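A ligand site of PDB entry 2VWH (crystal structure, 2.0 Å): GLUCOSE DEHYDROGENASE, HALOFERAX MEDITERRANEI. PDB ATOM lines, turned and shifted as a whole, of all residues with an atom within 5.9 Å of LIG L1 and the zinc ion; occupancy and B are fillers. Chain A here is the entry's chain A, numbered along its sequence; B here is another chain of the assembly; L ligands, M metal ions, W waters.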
ATOM      1  N   ASP A  38       5.509  13.656  10.273  1.00  0.00           N
ATOM      2  CA  ASP A  38       5.939  12.271  10.096  1.00  0.00           C
ATOM      3  C   ASP A  38       7.376  12.169   9.579  1.00  0.00           C
ATOM      4  O   ASP A  38       8.068  13.179   9.452  1.00  0.00           O
ATOM      5  CB  ASP A  38       4.920  11.437   9.281  1.00  0.00           C
ATOM      6  CG  ASP A  38       4.996  11.654   7.767  1.00  0.00           C
ATOM      7  OD1 ASP A  38       5.738  12.497   7.246  1.00  0.00           O
ATOM      8  OD2 ASP A  38       4.264  10.933   7.073  1.00  0.00           O
ATOM      9  N   THR A  40       8.461  11.404   6.655  1.00  0.00           N
ATOM     10  CA  THR A  40       8.628  12.070   5.348  1.00  0.00           C
ATOM     11  C   THR A  40       8.929  13.570   5.523  1.00  0.00           C
ATOM     12  O   THR A  40       9.785  14.117   4.833  1.00  0.00           O
ATOM     13  CB  THR A  40       7.392  11.832   4.446  1.00  0.00           C
ATOM     14  OG1 THR A  40       7.191  10.413   4.266  1.00  0.00           O
ATOM     15  CG2 THR A  40       7.564  12.502   3.084  1.00  0.00           C
ATOM     16  N   ASP A  41       8.245  14.223   6.445  1.00  0.00           N
ATOM     17  CA  ASP A  41       8.535  15.642   6.755  1.00  0.00           C
ATOM     18  C   ASP A  41       9.999  15.883   7.151  1.00  0.00           C
ATOM     19  O   ASP A  41      10.621  16.851   6.707  1.00  0.00           O
ATOM     20  CB  ASP A  41       7.624  16.174   7.875  1.00  0.00           C
ATOM     21  CG  ASP A  41       6.144  16.130   7.493  1.00  0.00           C
ATOM     22  OD1 ASP A  41       5.822  16.471   6.344  1.00  0.00           O
ATOM     23  OD2 ASP A  41       5.320  15.728   8.340  1.00  0.00           O
ATOM     24  N   HIS A  49      14.112  14.189   0.221  1.00  0.00           N
ATOM     25  CA  HIS A  49      12.873  13.904  -0.535  1.00  0.00           C
ATOM     26  C   HIS A  49      12.124  15.214  -0.792  1.00  0.00           C
ATOM     27  O   HIS A  49      12.201  16.157  -0.019  1.00  0.00           O
ATOM     28  CB  HIS A  49      11.990  12.903   0.238  1.00  0.00           C
ATOM     29  CG  HIS A  49      10.741  12.480  -0.480  1.00  0.00           C
ATOM     30  ND1 HIS A  49      10.755  11.673  -1.611  1.00  0.00           N
ATOM     31  CD2 HIS A  49       9.436  12.712  -0.218  1.00  0.00           C
ATOM     32  CE1 HIS A  49       9.512  11.453  -2.013  1.00  0.00           C
ATOM     33  NE2 HIS A  49       8.696  12.067  -1.178  1.00  0.00           N
ATOM     34  N   HIS A  63       1.663  17.979   5.755  1.00  0.00           N
ATOM     35  CA  HIS A  63       0.729  17.326   4.834  1.00  0.00           C
ATOM     36  C   HIS A  63      -0.393  16.537   5.530  1.00  0.00           C
ATOM     37  O   HIS A  63      -1.346  16.140   4.863  1.00  0.00           O
ATOM     38  CB  HIS A  63       1.496  16.440   3.829  1.00  0.00           C
ATOM     39  CG  HIS A  63       2.208  15.286   4.451  1.00  0.00           C
ATOM     40  ND1 HIS A  63       3.486  15.386   4.947  1.00  0.00           N
ATOM     41  CD2 HIS A  63       1.828  13.997   4.642  1.00  0.00           C
ATOM     42  CE1 HIS A  63       3.860  14.204   5.422  1.00  0.00           C
ATOM     43  NE2 HIS A  63       2.872  13.351   5.249  1.00  0.00           N
ATOM     44  N   GLU A  64      -0.280  16.326   6.848  1.00  0.00           N
ATOM     45  CA  GLU A  64      -1.283  15.624   7.641  1.00  0.00           C
ATOM     46  C   GLU A  64      -2.084  16.661   8.433  1.00  0.00           C
ATOM     47  O   GLU A  64      -1.660  17.082   9.496  1.00  0.00           O
ATOM     48  CB  GLU A  64      -0.611  14.681   8.647  1.00  0.00           C
ATOM     49  CG  GLU A  64       0.309  13.602   8.090  1.00  0.00           C
ATOM     50  CD  GLU A  64       0.980  12.758   9.181  1.00  0.00           C
ATOM     51  OE1 GLU A  64       1.052  13.218  10.343  1.00  0.00           O
ATOM     52  OE2 GLU A  64       1.436  11.624   8.884  1.00  0.00           O
ATOM     53  N   VAL A  87      -3.593  15.321  -0.337  1.00  0.00           N
ATOM     54  CA  VAL A  87      -2.248  15.875  -0.462  1.00  0.00           C
ATOM     55  C   VAL A  87      -1.863  16.279  -1.890  1.00  0.00           C
ATOM     56  O   VAL A  87      -1.194  17.316  -2.096  1.00  0.00           O
ATOM     57  CB  VAL A  87      -1.239  14.900   0.159  1.00  0.00           C
ATOM     58  CG1 VAL A  87       0.204  15.405  -0.032  1.00  0.00           C
ATOM     59  CG2 VAL A  87      -1.585  14.690   1.649  1.00  0.00           C
ATOM     60  N   ARG A  88      -2.326  15.518  -2.877  1.00  0.00           N
ATOM     61  CA  ARG A  88      -1.919  15.750  -4.274  1.00  0.00           C
ATOM     62  C   ARG A  88      -2.776  16.761  -5.027  1.00  0.00           C
ATOM     63  O   ARG A  88      -4.006  16.798  -4.881  1.00  0.00           O
ATOM     64  CB  ARG A  88      -1.845  14.422  -5.056  1.00  0.00           C
ATOM     65  CG  ARG A  88      -0.583  13.691  -4.735  1.00  0.00           C
ATOM     66  CD  ARG A  88      -0.419  12.415  -5.526  1.00  0.00           C
ATOM     67  NE  ARG A  88       0.827  11.765  -5.157  1.00  0.00           N
ATOM     68  CZ  ARG A  88       1.375  10.747  -5.821  1.00  0.00           C
ATOM     69  NH1 ARG A  88       0.763  10.234  -6.880  1.00  0.00           N
ATOM     70  NH2 ARG A  88       2.535  10.233  -5.421  1.00  0.00           N
ATOM     71  N   GLU A 114       2.692  17.480  -4.376  1.00  0.00           N
ATOM     72  CA  GLU A 114       2.206  17.102  -3.062  1.00  0.00           C
ATOM     73  C   GLU A 114       2.412  18.278  -2.116  1.00  0.00           C
ATOM     74  O   GLU A 114       3.546  18.735  -1.891  1.00  0.00           O
ATOM     75  CB  GLU A 114       2.948  15.871  -2.529  1.00  0.00           C
ATOM     76  CG  GLU A 114       2.540  14.584  -3.217  1.00  0.00           C
ATOM     77  CD  GLU A 114       3.374  13.350  -2.803  1.00  0.00           C
ATOM     78  OE1 GLU A 114       4.482  13.467  -2.222  1.00  0.00           O
ATOM     79  OE2 GLU A 114       2.905  12.231  -3.099  1.00  0.00           O
ATOM     80  N   ILE A 117       5.340  18.826   0.496  1.00  0.00           N
ATOM     81  CA  ILE A 117       6.337  17.824   0.173  1.00  0.00           C
ATOM     82  C   ILE A 117       7.046  18.137  -1.140  1.00  0.00           C
ATOM     83  O   ILE A 117       8.260  18.283  -1.167  1.00  0.00           O
ATOM     84  CB  ILE A 117       5.752  16.391   0.120  1.00  0.00           C
ATOM     85  CG1 ILE A 117       5.035  16.042   1.437  1.00  0.00           C
ATOM     86  CG2 ILE A 117       6.884  15.358  -0.121  1.00  0.00           C
ATOM     87  CD1 ILE A 117       4.345  14.668   1.414  1.00  0.00           C
ATOM     88  N   GLU A 150      -5.013  11.073   7.515  1.00  0.00           N
ATOM     89  CA  GLU A 150      -4.119  10.911   6.366  1.00  0.00           C
ATOM     90  C   GLU A 150      -3.233   9.662   6.441  1.00  0.00           C
ATOM     91  O   GLU A 150      -3.237   8.861   5.501  1.00  0.00           O
ATOM     92  CB  GLU A 150      -3.319  12.198   6.093  1.00  0.00           C
ATOM     93  CG  GLU A 150      -2.639  12.238   4.720  1.00  0.00           C
ATOM     94  CD  GLU A 150      -1.265  11.608   4.689  1.00  0.00           C
ATOM     95  OE1 GLU A 150      -0.755  11.250   5.769  1.00  0.00           O
ATOM     96  OE2 GLU A 150      -0.696  11.483   3.577  1.00  0.00           O
ATOM     97  N   PRO A 151      -2.446   9.497   7.519  1.00  0.00           N
ATOM     98  CA  PRO A 151      -1.619   8.262   7.575  1.00  0.00           C
ATOM     99  C   PRO A 151      -2.416   6.950   7.619  1.00  0.00           C
ATOM    100  O   PRO A 151      -1.977   5.958   7.039  1.00  0.00           O
ATOM    101  CB  PRO A 151      -0.756   8.447   8.837  1.00  0.00           C
ATOM    102  CG  PRO A 151      -1.408   9.545   9.619  1.00  0.00           C
ATOM    103  CD  PRO A 151      -2.140  10.413   8.645  1.00  0.00           C
ATOM    104  N   ILE A 154      -3.195   6.066   4.030  1.00  0.00           N
ATOM    105  CA  ILE A 154      -2.073   5.464   3.351  1.00  0.00           C
ATOM    106  C   ILE A 154      -2.166   3.930   3.428  1.00  0.00           C
ATOM    107  O   ILE A 154      -2.064   3.230   2.413  1.00  0.00           O
ATOM    108  CB  ILE A 154      -0.725   5.926   3.967  1.00  0.00           C
ATOM    109  CG1 ILE A 154      -0.513   7.442   3.801  1.00  0.00           C
ATOM    110  CG2 ILE A 154       0.464   5.120   3.379  1.00  0.00           C
ATOM    111  CD1 ILE A 154      -0.419   7.946   2.347  1.00  0.00           C
ATOM    112  N   VAL A 274      10.060   5.180   1.835  1.00  0.00           N
ATOM    113  CA  VAL A 274      10.773   6.034   0.878  1.00  0.00           C
ATOM    114  C   VAL A 274      12.269   5.853   1.150  1.00  0.00           C
ATOM    115  O   VAL A 274      12.796   6.317   2.161  1.00  0.00           O
ATOM    116  CB  VAL A 274      10.356   7.502   0.999  1.00  0.00           C
ATOM    117  CG1 VAL A 274      11.168   8.380   0.046  1.00  0.00           C
ATOM    118  CG2 VAL A 274       8.842   7.649   0.715  1.00  0.00           C
ATOM    119  N   VAL A 302       1.938   4.270  -2.829  1.00  0.00           N
ATOM    120  CA  VAL A 302       2.226   5.627  -2.374  1.00  0.00           C
ATOM    121  C   VAL A 302       0.973   6.478  -2.400  1.00  0.00           C
ATOM    122  O   VAL A 302       0.104   6.291  -3.264  1.00  0.00           O
ATOM    123  CB  VAL A 302       3.382   6.299  -3.191  1.00  0.00           C
ATOM    124  CG1 VAL A 302       2.951   6.591  -4.667  1.00  0.00           C
ATOM    125  CG2 VAL A 302       3.860   7.573  -2.497  1.00  0.00           C
ATOM    126  N   ASN A 303       0.861   7.380  -1.427  1.00  0.00           N
ATOM    127  CA  ASN A 303      -0.219   8.359  -1.399  1.00  0.00           C
ATOM    128  C   ASN A 303      -1.551   7.648  -1.164  1.00  0.00           C
ATOM    129  O   ASN A 303      -1.576   6.492  -0.717  1.00  0.00           O
ATOM    130  CB  ASN A 303      -0.198   9.204  -2.690  1.00  0.00           C
ATOM    131  CG  ASN A 303      -1.001  10.491  -2.591  1.00  0.00           C
ATOM    132  OD1 ASN A 303      -1.982  10.666  -3.315  1.00  0.00           O
ATOM    133  ND2 ASN A 303      -0.624  11.384  -1.688  1.00  0.00           N
ATOM    134  N   SER A 304      -2.655   8.339  -1.446  1.00  0.00           N
ATOM    135  CA  SER A 304      -3.993   7.811  -1.197  1.00  0.00           C
ATOM    136  C   SER A 304      -4.965   8.863  -1.694  1.00  0.00           C
ATOM    137  O   SER A 304      -4.574  10.002  -1.967  1.00  0.00           O
ATOM    138  CB  SER A 304      -4.246   7.541   0.290  1.00  0.00           C
ATOM    139  OG  SER A 304      -4.054   8.707   1.069  1.00  0.00           O
ATOM    140  N   LEU B 293       7.329   4.480  -5.202  1.00  0.00           N
ATOM    141  CA  LEU B 293       6.917   5.785  -5.735  1.00  0.00           C
ATOM    142  C   LEU B 293       6.116   5.689  -7.027  1.00  0.00           C
ATOM    143  O   LEU B 293       5.415   6.640  -7.393  1.00  0.00           O
ATOM    144  CB  LEU B 293       8.139   6.702  -5.921  1.00  0.00           C
ATOM    145  CG  LEU B 293       8.851   7.135  -4.624  1.00  0.00           C
ATOM    146  CD1 LEU B 293      10.064   8.010  -4.921  1.00  0.00           C
ATOM    147  CD2 LEU B 293       7.912   7.872  -3.683  1.00  0.00           C
HETATM  148  C1  LIG L   1       2.545  11.340   2.467  1.00  0.00           C
HETATM  149  C2  LIG L   1       1.945  10.832   1.168  1.00  0.00           C
HETATM  150  C3  LIG L   1       2.998  10.968   0.086  1.00  0.00           C
HETATM  151  C4  LIG L   1       4.302  10.238   0.504  1.00  0.00           C
HETATM  152  C5  LIG L   1       5.366  10.383  -0.598  1.00  0.00           C
HETATM  153  C6  LIG L   1       3.829  10.602   2.783  1.00  0.00           C
HETATM  154  O1  LIG L   1       4.232  10.992   4.069  1.00  0.00           O
HETATM  155  O2  LIG L   1       1.694  10.930   3.503  1.00  0.00           O
HETATM  156  O3  LIG L   1       0.783  11.581   0.843  1.00  0.00           O
HETATM  157  O4  LIG L   1       2.480  10.529  -1.143  1.00  0.00           O
HETATM  158  O5  LIG L   1       4.785  10.745   1.763  1.00  0.00           O
HETATM  159  O6  LIG L   1       5.760  11.724  -0.634  1.00  0.00           O
HETATM  160  P1  LG2 L   2       9.846   6.959  10.774  1.00  0.00           P
HETATM  161  O1  LG2 L   2       9.280   7.706  11.921  1.00  0.00           O
HETATM  162  O2  LG2 L   2      11.156   7.374  10.315  1.00  0.00           O
HETATM  163  O3  LG2 L   2       9.837   5.412  11.149  1.00  0.00           O
HETATM  164  C1  LG2 L   2      10.757   4.521  10.550  1.00  0.00           C
HETATM  165  C2  LG2 L   2      11.152   3.528  11.619  1.00  0.00           C
HETATM  166  O4  LG2 L   2      11.855   2.460  11.029  1.00  0.00           O
HETATM  167  C3  LG2 L   2      12.064   4.164  12.672  1.00  0.00           C
HETATM  168  O5  LG2 L   2      11.425   4.140  13.929  1.00  0.00           O
HETATM  169  C4  LG2 L   2      13.313   3.310  12.633  1.00  0.00           C
HETATM  170  O6  LG2 L   2      13.793   3.007  13.914  1.00  0.00           O
HETATM  171  C5  LG2 L   2      12.845   2.044  11.934  1.00  0.00           C
HETATM  172  N1  LG2 L   2      13.977   1.369  11.280  1.00  0.00           N
HETATM  173  C6  LG2 L   2      14.818   1.894  10.316  1.00  0.00           C
HETATM  174  N2  LG2 L   2      15.724   0.953   9.996  1.00  0.00           N
HETATM  175  C7  LG2 L   2      15.487  -0.148  10.756  1.00  0.00           C
HETATM  176  C8  LG2 L   2      16.122  -1.376  10.824  1.00  0.00           C
HETATM  177  N3  LG2 L   2      17.175  -1.633  10.053  1.00  0.00           N
HETATM  178  N4  LG2 L   2      15.641  -2.330  11.694  1.00  0.00           N
HETATM  179  C9  LG2 L   2      14.526  -2.069  12.482  1.00  0.00           C
HETATM  180  N5  LG2 L   2      13.903  -0.840  12.401  1.00  0.00           N
HETATM  181  C10 LG2 L   2      14.382   0.098  11.558  1.00  0.00           C
HETATM  182  O7  LG2 L   2       8.813   7.086   9.543  1.00  0.00           O
HETATM  183  P2  LG2 L   2       7.217   6.916   9.468  1.00  0.00           P
HETATM  184  O8  LG2 L   2       6.755   5.832  10.373  1.00  0.00           O
HETATM  185  O9  LG2 L   2       6.558   8.247   9.520  1.00  0.00           O
HETATM  186  O10 LG2 L   2       7.140   6.369   7.958  1.00  0.00           O
HETATM  187  C11 LG2 L   2       7.726   5.146   7.580  1.00  0.00           C
HETATM  188  C12 LG2 L   2       8.327   5.200   6.186  1.00  0.00           C
HETATM  189  O11 LG2 L   2       7.288   5.319   5.238  1.00  0.00           O
HETATM  190  C13 LG2 L   2       9.262   6.365   5.887  1.00  0.00           C
HETATM  191  O12 LG2 L   2      10.225   5.948   4.938  1.00  0.00           O
HETATM  192  C14 LG2 L   2       8.339   7.403   5.300  1.00  0.00           C
HETATM  193  O13 LG2 L   2       8.972   8.369   4.516  1.00  0.00           O
HETATM  194  C15 LG2 L   2       7.433   6.517   4.463  1.00  0.00           C
HETATM  195  N6  LG2 L   2       6.062   6.995   4.176  1.00  0.00           N
HETATM  196  C16 LG2 L   2       5.583   6.693   2.926  1.00  0.00           C
HETATM  197  C17 LG2 L   2       4.295   7.016   2.555  1.00  0.00           C
HETATM  198  C18 LG2 L   2       3.776   6.453   1.260  1.00  0.00           C
HETATM  199  O14 LG2 L   2       2.637   7.064   0.712  1.00  0.00           O
HETATM  200  N7  LG2 L   2       4.370   5.419   0.641  1.00  0.00           N
HETATM  201  C19 LG2 L   2       3.471   7.680   3.466  1.00  0.00           C
HETATM  202  C20 LG2 L   2       3.966   7.943   4.764  1.00  0.00           C
HETATM  203  C21 LG2 L   2       5.267   7.601   5.113  1.00  0.00           C
HETATM  204  P3  LG2 L   2      14.866   3.954  14.664  1.00  0.00           P
HETATM  205  O15 LG2 L   2      14.149   5.157  15.164  1.00  0.00           O
HETATM  206  O16 LG2 L   2      15.959   4.349  13.735  1.00  0.00           O
HETATM  207  O17 LG2 L   2      15.381   3.123  15.807  1.00  0.00           O
HETATM  208 ZN    ZN M   1       2.976  11.405   5.582  1.00  0.00          ZN
HETATM  209  O   HOH W   1      -2.300  10.848   1.229  1.00  0.00           O
HETATM  210  O   HOH W   2       1.431  10.758   6.571  1.00  0.00           O
HETATM  211  O   HOH W   3       6.374  11.755  -3.766  1.00  0.00           O
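The side-chain amide nitrogen (ND2) of Asn 303 is in hydrogen-bond range of an oxygen (O3) of LIG L1, at 2.9 Å.
NE2 of His 49 sits at hydrogen-bond distance from O6 of LIG L1 (3.0 Å).
O14 of LG2 L2 sits at hydrogen-bond distance from N of Asn 303, 2.8 Å away.
OG1 of Thr 40 is in hydrogen-bond range of O5 of LIG L1.
The side-chain carboxylate (OE2) of Glu 150 lies within hydrogen-bond range of an oxygen (O3) of LIG L1, at 3.1 Å.
OG1 of Thr 40 is in hydrogen-bond range of O13 of LG2 L2, 2.7 Å away.
The side-chain carboxylate (OE2) of Glu 114 lies within hydrogen-bond range of an oxygen (O4) of LIG L1, at 2.6 Å.
An oxygen (O12) of LG2 L2 is in hydrogen-bond range of the backbone NH (N) of Val 274 (3.2 Å).
OE2 of Glu 114 is in salt-bridge range of NE of Arg 88 (3.0 Å).
ND1 of His 63 lies within hydrogen-bond range of OD1 of Asp 41, at 2.9 Å.
The backbone NH of Asp 38 lies within hydrogen-bond range of the side-chain carboxylate of Asp 41 (2.8 Å).
The side-chain carboxylate (OD1) of Asp 38 sits at hydrogen-bond distance from the backbone NH (N) of Thr 40 (3.0 Å).
Residues that only touch LIG L1: Val 87 (3.9 Å), Ile 117 (3.8 Å), Ile 154 (3.8 Å) and Val 302 (3.5 Å).
Hydrophobic or aromatic side chains that line LIG L1: His 49, His 63, Val 87, Ile 117, Ile 154 and Val 302.
11 residues have an atom within 4 Å of LIG L1: Asp 38, Thr 40, His 49, His 63, Val 87, Glu 114, Ile 117, Glu 150, Ile 154, Val 302 and Asn 303.
Glu 64 touches the zinc ion.
Glu 150 touches the zinc ion.
Within 4 Å of the zinc ion: Asp 38, His 63, Glu 64 and Glu 150.
Along chain A the residues within 4 Å of the zinc ion span positions 38 to 150.
The zinc ion is bound by water W2, a ring nitrogen (NE2) of His 63, an oxygen (O1) of LIG L1, the side-chain carboxylate (OD2) of Asp 38 and an oxygen (O2) of LIG L1.
Water W3 lies within hydrogen-bond range of OE1 of Glu 114, O6 of LIG L1 and NE2 of His 49.
Water W1 lies within hydrogen-bond range of OG of Ser 304, OE2 of Glu 150, O3 of LIG L1 and ND2 of Asn 303.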
